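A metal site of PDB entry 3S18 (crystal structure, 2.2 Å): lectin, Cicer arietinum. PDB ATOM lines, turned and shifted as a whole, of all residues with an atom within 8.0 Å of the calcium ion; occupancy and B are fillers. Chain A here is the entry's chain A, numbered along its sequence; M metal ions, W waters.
O of Phe 21 lies within hydrogen-bond range of N of Asn 7, 2.8 Å away.
The backbone NH of Asp 65 lies within hydrogen-bond range of the backbone carbonyl oxygen of Phe 78, at 2.9 Å.
The backbone carbonyl oxygen (O) of Phe 135 lies within hydrogen-bond range of the backbone NH (N) of Asp 121 (2.8 Å).
The backbone carbonyl oxygen (O) of Phe 188 is in hydrogen-bond range of the backbone NH (N) of Asp 174, at 2.9 Å.
The calcium ion is bound by water W2 (2.2 Å), O of Asn 7 (2.3 Å), O of Asp 65 (2.4 Å), water W1 (2.4 Å), O of Asp 121 (2.4 Å), OD1 of Asn 7 (2.4 Å) and O of Asp 174 (2.4 Å).
The calcium ion has seven donor atoms within binding distance.
Four residues have an atom within 4 Å of the calcium ion: Asn 7, Asp 65, Asp 121 and Asp 174.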
ATOM      1  N   TYR A   5      38.469  -9.905  -4.755  1.00  0.00           N
ATOM      2  CA  TYR A   5      38.005  -8.732  -5.468  1.00  0.00           C
ATOM      3  C   TYR A   5      36.558  -8.374  -5.077  1.00  0.00           C
ATOM      4  O   TYR A   5      35.995  -9.013  -4.187  1.00  0.00           O
ATOM      5  CB  TYR A   5      38.140  -8.963  -6.977  1.00  0.00           C
ATOM      6  CG  TYR A   5      39.578  -8.989  -7.449  1.00  0.00           C
ATOM      7  CD1 TYR A   5      40.259  -7.795  -7.713  1.00  0.00           C
ATOM      8  CD2 TYR A   5      40.268 -10.191  -7.604  1.00  0.00           C
ATOM      9  CE1 TYR A   5      41.594  -7.803  -8.152  1.00  0.00           C
ATOM     10  CE2 TYR A   5      41.605 -10.218  -8.037  1.00  0.00           C
ATOM     11  CZ  TYR A   5      42.257  -9.020  -8.310  1.00  0.00           C
ATOM     12  OH  TYR A   5      43.572  -9.048  -8.739  1.00  0.00           O
ATOM     13  N   ILE A   6      35.992  -7.359  -5.714  1.00  0.00           N
ATOM     14  CA  ILE A   6      34.605  -6.939  -5.461  1.00  0.00           C
ATOM     15  C   ILE A   6      33.627  -8.100  -5.691  1.00  0.00           C
ATOM     16  O   ILE A   6      33.562  -8.622  -6.798  1.00  0.00           O
ATOM     17  CB  ILE A   6      34.215  -5.705  -6.329  1.00  0.00           C
ATOM     18  CG1 ILE A   6      35.190  -4.558  -6.076  1.00  0.00           C
ATOM     19  CG2 ILE A   6      32.775  -5.260  -6.042  1.00  0.00           C
ATOM     20  CD1 ILE A   6      35.221  -3.532  -7.159  1.00  0.00           C
ATOM     21  N   ASN A   7      32.899  -8.499  -4.655  1.00  0.00           N
ATOM     22  CA  ASN A   7      31.975  -9.648  -4.704  1.00  0.00           C
ATOM     23  C   ASN A   7      30.510  -9.258  -4.844  1.00  0.00           C
ATOM     24  O   ASN A   7      29.686 -10.033  -5.329  1.00  0.00           O
ATOM     25  CB  ASN A   7      32.154 -10.523  -3.457  1.00  0.00           C
ATOM     26  CG  ASN A   7      31.719 -11.990  -3.658  1.00  0.00           C
ATOM     27  OD1 ASN A   7      31.174 -12.401  -4.689  1.00  0.00           O
ATOM     28  ND2 ASN A   7      31.949 -12.799  -2.614  1.00  0.00           N
ATOM     29  N   ALA A   8      30.171  -8.034  -4.407  1.00  0.00           N
ATOM     30  CA  ALA A   8      28.821  -7.488  -4.481  1.00  0.00           C
ATOM     31  C   ALA A   8      28.872  -5.956  -4.380  1.00  0.00           C
ATOM     32  O   ALA A   8      29.862  -5.398  -3.918  1.00  0.00           O
ATOM     33  CB  ALA A   8      27.927  -8.068  -3.348  1.00  0.00           C
ATOM     34  N   ALA A   9      27.780  -5.303  -4.786  1.00  0.00           N
ATOM     35  CA  ALA A   9      27.631  -3.841  -4.707  1.00  0.00           C
ATOM     36  C   ALA A   9      26.160  -3.457  -4.868  1.00  0.00           C
ATOM     37  O   ALA A   9      25.362  -4.230  -5.431  1.00  0.00           O
ATOM     38  CB  ALA A   9      28.477  -3.153  -5.804  1.00  0.00           C
ATOM     39  N   PHE A  21      31.247  -4.612  -1.605  1.00  0.00           N
ATOM     40  CA  PHE A  21      31.546  -5.665  -0.644  1.00  0.00           C
ATOM     41  C   PHE A  21      32.685  -6.549  -1.123  1.00  0.00           C
ATOM     42  O   PHE A  21      32.684  -7.041  -2.264  1.00  0.00           O
ATOM     43  CB  PHE A  21      30.272  -6.476  -0.333  1.00  0.00           C
ATOM     44  CG  PHE A  21      29.156  -5.624   0.212  1.00  0.00           C
ATOM     45  CD1 PHE A  21      28.999  -5.462   1.584  1.00  0.00           C
ATOM     46  CD2 PHE A  21      28.306  -4.920  -0.653  1.00  0.00           C
ATOM     47  CE1 PHE A  21      28.014  -4.623   2.102  1.00  0.00           C
ATOM     48  CE2 PHE A  21      27.317  -4.087  -0.157  1.00  0.00           C
ATOM     49  CZ  PHE A  21      27.159  -3.943   1.230  1.00  0.00           C
ATOM     50  N   ILE A  64      28.912 -10.550   2.102  1.00  0.00           N
ATOM     51  CA  ILE A  64      27.778 -10.460   1.207  1.00  0.00           C
ATOM     52  C   ILE A  64      28.245 -10.736  -0.219  1.00  0.00           C
ATOM     53  O   ILE A  64      29.093 -10.012  -0.753  1.00  0.00           O
ATOM     54  CB  ILE A  64      27.131  -9.052   1.333  1.00  0.00           C
ATOM     55  CG1 ILE A  64      26.397  -8.932   2.677  1.00  0.00           C
ATOM     56  CG2 ILE A  64      26.188  -8.757   0.151  1.00  0.00           C
ATOM     57  CD1 ILE A  64      26.287  -7.470   3.210  1.00  0.00           C
ATOM     58  N   ASP A  65      27.725 -11.786  -0.848  1.00  0.00           N
ATOM     59  CA  ASP A  65      28.258 -12.159  -2.160  1.00  0.00           C
ATOM     60  C   ASP A  65      27.406 -11.728  -3.342  1.00  0.00           C
ATOM     61  O   ASP A  65      27.804 -11.929  -4.496  1.00  0.00           O
ATOM     62  CB  ASP A  65      28.629 -13.666  -2.226  1.00  0.00           C
ATOM     63  CG  ASP A  65      27.429 -14.559  -2.099  1.00  0.00           C
ATOM     64  OD1 ASP A  65      26.281 -14.141  -2.346  1.00  0.00           O
ATOM     65  OD2 ASP A  65      27.625 -15.724  -1.750  1.00  0.00           O
ATOM     66  N   CYS A  66      26.253 -11.128  -3.063  1.00  0.00           N
ATOM     67  CA  CYS A  66      25.415 -10.532  -4.101  1.00  0.00           C
ATOM     68  C   CYS A  66      24.489  -9.526  -3.450  1.00  0.00           C
ATOM     69  O   CYS A  66      24.115  -9.700  -2.306  1.00  0.00           O
ATOM     70  CB  CYS A  66      24.577 -11.585  -4.840  1.00  0.00           C
ATOM     71  SG  CYS A  66      23.600 -10.990  -6.251  1.00  0.00           S
ATOM     72  N   SER A  67      24.158  -8.464  -4.167  1.00  0.00           N
ATOM     73  CA  SER A  67      23.054  -7.600  -3.738  1.00  0.00           C
ATOM     74  C   SER A  67      22.570  -6.634  -4.788  1.00  0.00           C
ATOM     75  O   SER A  67      23.149  -6.533  -5.863  1.00  0.00           O
ATOM     76  CB  SER A  67      23.343  -6.875  -2.433  1.00  0.00           C
ATOM     77  OG  SER A  67      24.498  -6.097  -2.544  1.00  0.00           O
ATOM     78  N   PHE A  78      22.747 -11.023  -0.130  1.00  0.00           N
ATOM     79  CA  PHE A  78      22.828 -12.480  -0.279  1.00  0.00           C
ATOM     80  C   PHE A  78      24.111 -13.040   0.279  1.00  0.00           C
ATOM     81  O   PHE A  78      25.127 -12.363   0.316  1.00  0.00           O
ATOM     82  CB  PHE A  78      22.773 -12.868  -1.745  1.00  0.00           C
ATOM     83  CG  PHE A  78      21.493 -12.522  -2.441  1.00  0.00           C
ATOM     84  CD1 PHE A  78      20.520 -13.507  -2.638  1.00  0.00           C
ATOM     85  CD2 PHE A  78      21.291 -11.245  -2.955  1.00  0.00           C
ATOM     86  CE1 PHE A  78      19.319 -13.213  -3.324  1.00  0.00           C
ATOM     87  CE2 PHE A  78      20.084 -10.919  -3.640  1.00  0.00           C
ATOM     88  CZ  PHE A  78      19.101 -11.923  -3.823  1.00  0.00           C
ATOM     89  N   ILE A 120      23.596 -16.551  -6.096  1.00  0.00           N
ATOM     90  CA  ILE A 120      23.574 -15.638  -7.230  1.00  0.00           C
ATOM     91  C   ILE A 120      24.918 -14.887  -7.287  1.00  0.00           C
ATOM     92  O   ILE A 120      25.465 -14.496  -6.251  1.00  0.00           O
ATOM     93  CB  ILE A 120      22.338 -14.654  -7.116  1.00  0.00           C
ATOM     94  CG1 ILE A 120      21.055 -15.471  -6.901  1.00  0.00           C
ATOM     95  CG2 ILE A 120      22.227 -13.741  -8.367  1.00  0.00           C
ATOM     96  CD1 ILE A 120      19.753 -14.708  -6.687  1.00  0.00           C
ATOM     97  N   ASP A 121      25.459 -14.692  -8.501  1.00  0.00           N
ATOM     98  CA  ASP A 121      26.767 -14.025  -8.663  1.00  0.00           C
ATOM     99  C   ASP A 121      26.702 -12.515  -8.480  1.00  0.00           C
ATOM    100  O   ASP A 121      27.524 -11.933  -7.780  1.00  0.00           O
ATOM    101  CB  ASP A 121      27.384 -14.324 -10.046  1.00  0.00           C
ATOM    102  CG  ASP A 121      27.838 -15.765 -10.213  1.00  0.00           C
ATOM    103  OD1 ASP A 121      28.109 -16.455  -9.209  1.00  0.00           O
ATOM    104  OD2 ASP A 121      27.918 -16.229 -11.362  1.00  0.00           O
ATOM    105  N   ALA A 122      25.731 -11.869  -9.119  1.00  0.00           N
ATOM    106  CA  ALA A 122      25.662 -10.404  -9.179  1.00  0.00           C
ATOM    107  C   ALA A 122      24.267 -10.044  -9.580  1.00  0.00           C
ATOM    108  O   ALA A 122      23.493 -10.901 -10.043  1.00  0.00           O
ATOM    109  CB  ALA A 122      26.636  -9.846 -10.234  1.00  0.00           C
ATOM    110  N   ALA A 123      23.936  -8.767  -9.375  1.00  0.00           N
ATOM    111  CA  ALA A 123      22.629  -8.242  -9.741  1.00  0.00           C
ATOM    112  C   ALA A 123      22.715  -6.731  -9.890  1.00  0.00           C
ATOM    113  O   ALA A 123      23.565  -6.085  -9.273  1.00  0.00           O
ATOM    114  CB  ALA A 123      21.582  -8.610  -8.686  1.00  0.00           C
ATOM    115  N   PHE A 135      22.474 -12.420 -12.175  1.00  0.00           N
ATOM    116  CA  PHE A 135      23.403 -13.195 -12.976  1.00  0.00           C
ATOM    117  C   PHE A 135      23.934 -14.380 -12.180  1.00  0.00           C
ATOM    118  O   PHE A 135      24.203 -14.257 -10.979  1.00  0.00           O
ATOM    119  CB  PHE A 135      24.571 -12.300 -13.397  1.00  0.00           C
ATOM    120  CG  PHE A 135      24.148 -11.083 -14.195  1.00  0.00           C
ATOM    121  CD1 PHE A 135      24.047 -11.154 -15.589  1.00  0.00           C
ATOM    122  CD2 PHE A 135      23.867  -9.885 -13.567  1.00  0.00           C
ATOM    123  CE1 PHE A 135      23.661 -10.043 -16.331  1.00  0.00           C
ATOM    124  CE2 PHE A 135      23.490  -8.752 -14.313  1.00  0.00           C
ATOM    125  CZ  PHE A 135      23.390  -8.843 -15.702  1.00  0.00           C
ATOM    126  N   MET A 173      29.800 -12.826 -14.269  1.00  0.00           N
ATOM    127  CA  MET A 173      30.371 -11.644 -13.595  1.00  0.00           C
ATOM    128  C   MET A 173      30.255 -11.694 -12.099  1.00  0.00           C
ATOM    129  O   MET A 173      29.308 -12.263 -11.564  1.00  0.00           O
ATOM    130  CB  MET A 173      29.801 -10.338 -14.155  1.00  0.00           C
ATOM    131  CG  MET A 173      28.340 -10.247 -14.169  1.00  0.00           C
ATOM    132  SD  MET A 173      27.860  -9.551 -15.766  1.00  0.00           S
ATOM    133  CE  MET A 173      28.647 -10.705 -16.871  1.00  0.00           C
ATOM    134  N   ASP A 174      31.237 -11.101 -11.426  1.00  0.00           N
ATOM    135  CA  ASP A 174      31.416 -11.237  -9.985  1.00  0.00           C
ATOM    136  C   ASP A 174      30.554 -10.281  -9.158  1.00  0.00           C
ATOM    137  O   ASP A 174      30.160 -10.601  -8.047  1.00  0.00           O
ATOM    138  CB  ASP A 174      32.898 -11.103  -9.606  1.00  0.00           C
ATOM    139  CG  ASP A 174      33.714 -12.347  -9.931  1.00  0.00           C
ATOM    140  OD1 ASP A 174      33.070 -13.390 -10.170  1.00  0.00           O
ATOM    141  OD2 ASP A 174      34.994 -12.292  -9.955  1.00  0.00           O
ATOM    142  N   SER A 175      30.301  -9.099  -9.694  1.00  0.00           N
ATOM    143  CA  SER A 175      29.469  -8.118  -8.982  1.00  0.00           C
ATOM    144  C   SER A 175      29.042  -7.047  -9.936  1.00  0.00           C
ATOM    145  O   SER A 175      29.594  -6.953 -11.028  1.00  0.00           O
ATOM    146  CB  SER A 175      30.223  -7.497  -7.833  1.00  0.00           C
ATOM    147  OG  SER A 175      31.444  -6.966  -8.312  1.00  0.00           O
ATOM    148  N   ALA A 176      28.055  -6.248  -9.526  1.00  0.00           N
ATOM    149  CA  ALA A 176      27.486  -5.178 -10.347  1.00  0.00           C
ATOM    150  C   ALA A 176      26.681  -4.219  -9.496  1.00  0.00           C
ATOM    151  O   ALA A 176      26.204  -4.583  -8.396  1.00  0.00           O
ATOM    152  CB  ALA A 176      26.584  -5.764 -11.456  1.00  0.00           C
ATOM    153  N   PHE A 188      31.769  -6.016 -12.690  1.00  0.00           N
ATOM    154  CA  PHE A 188      33.116  -6.336 -12.237  1.00  0.00           C
ATOM    155  C   PHE A 188      33.436  -7.804 -12.335  1.00  0.00           C
ATOM    156  O   PHE A 188      32.564  -8.659 -12.125  1.00  0.00           O
ATOM    157  CB  PHE A 188      33.330  -5.876 -10.802  1.00  0.00           C
ATOM    158  CG  PHE A 188      33.113  -4.418 -10.591  1.00  0.00           C
ATOM    159  CD1 PHE A 188      34.162  -3.525 -10.735  1.00  0.00           C
ATOM    160  CD2 PHE A 188      31.852  -3.938 -10.247  1.00  0.00           C
ATOM    161  CE1 PHE A 188      33.962  -2.136 -10.556  1.00  0.00           C
ATOM    162  CE2 PHE A 188      31.634  -2.568 -10.057  1.00  0.00           C
ATOM    163  CZ  PHE A 188      32.693  -1.667 -10.211  1.00  0.00           C
HETATM  164 CA    CA M   1      29.385 -12.058  -6.273  1.00  0.00          CA
HETATM  165  O   HOH W   1      28.716 -14.247  -5.609  1.00  0.00           O
HETATM  166  O   HOH W   2      30.604 -13.659  -7.248  1.00  0.00           O
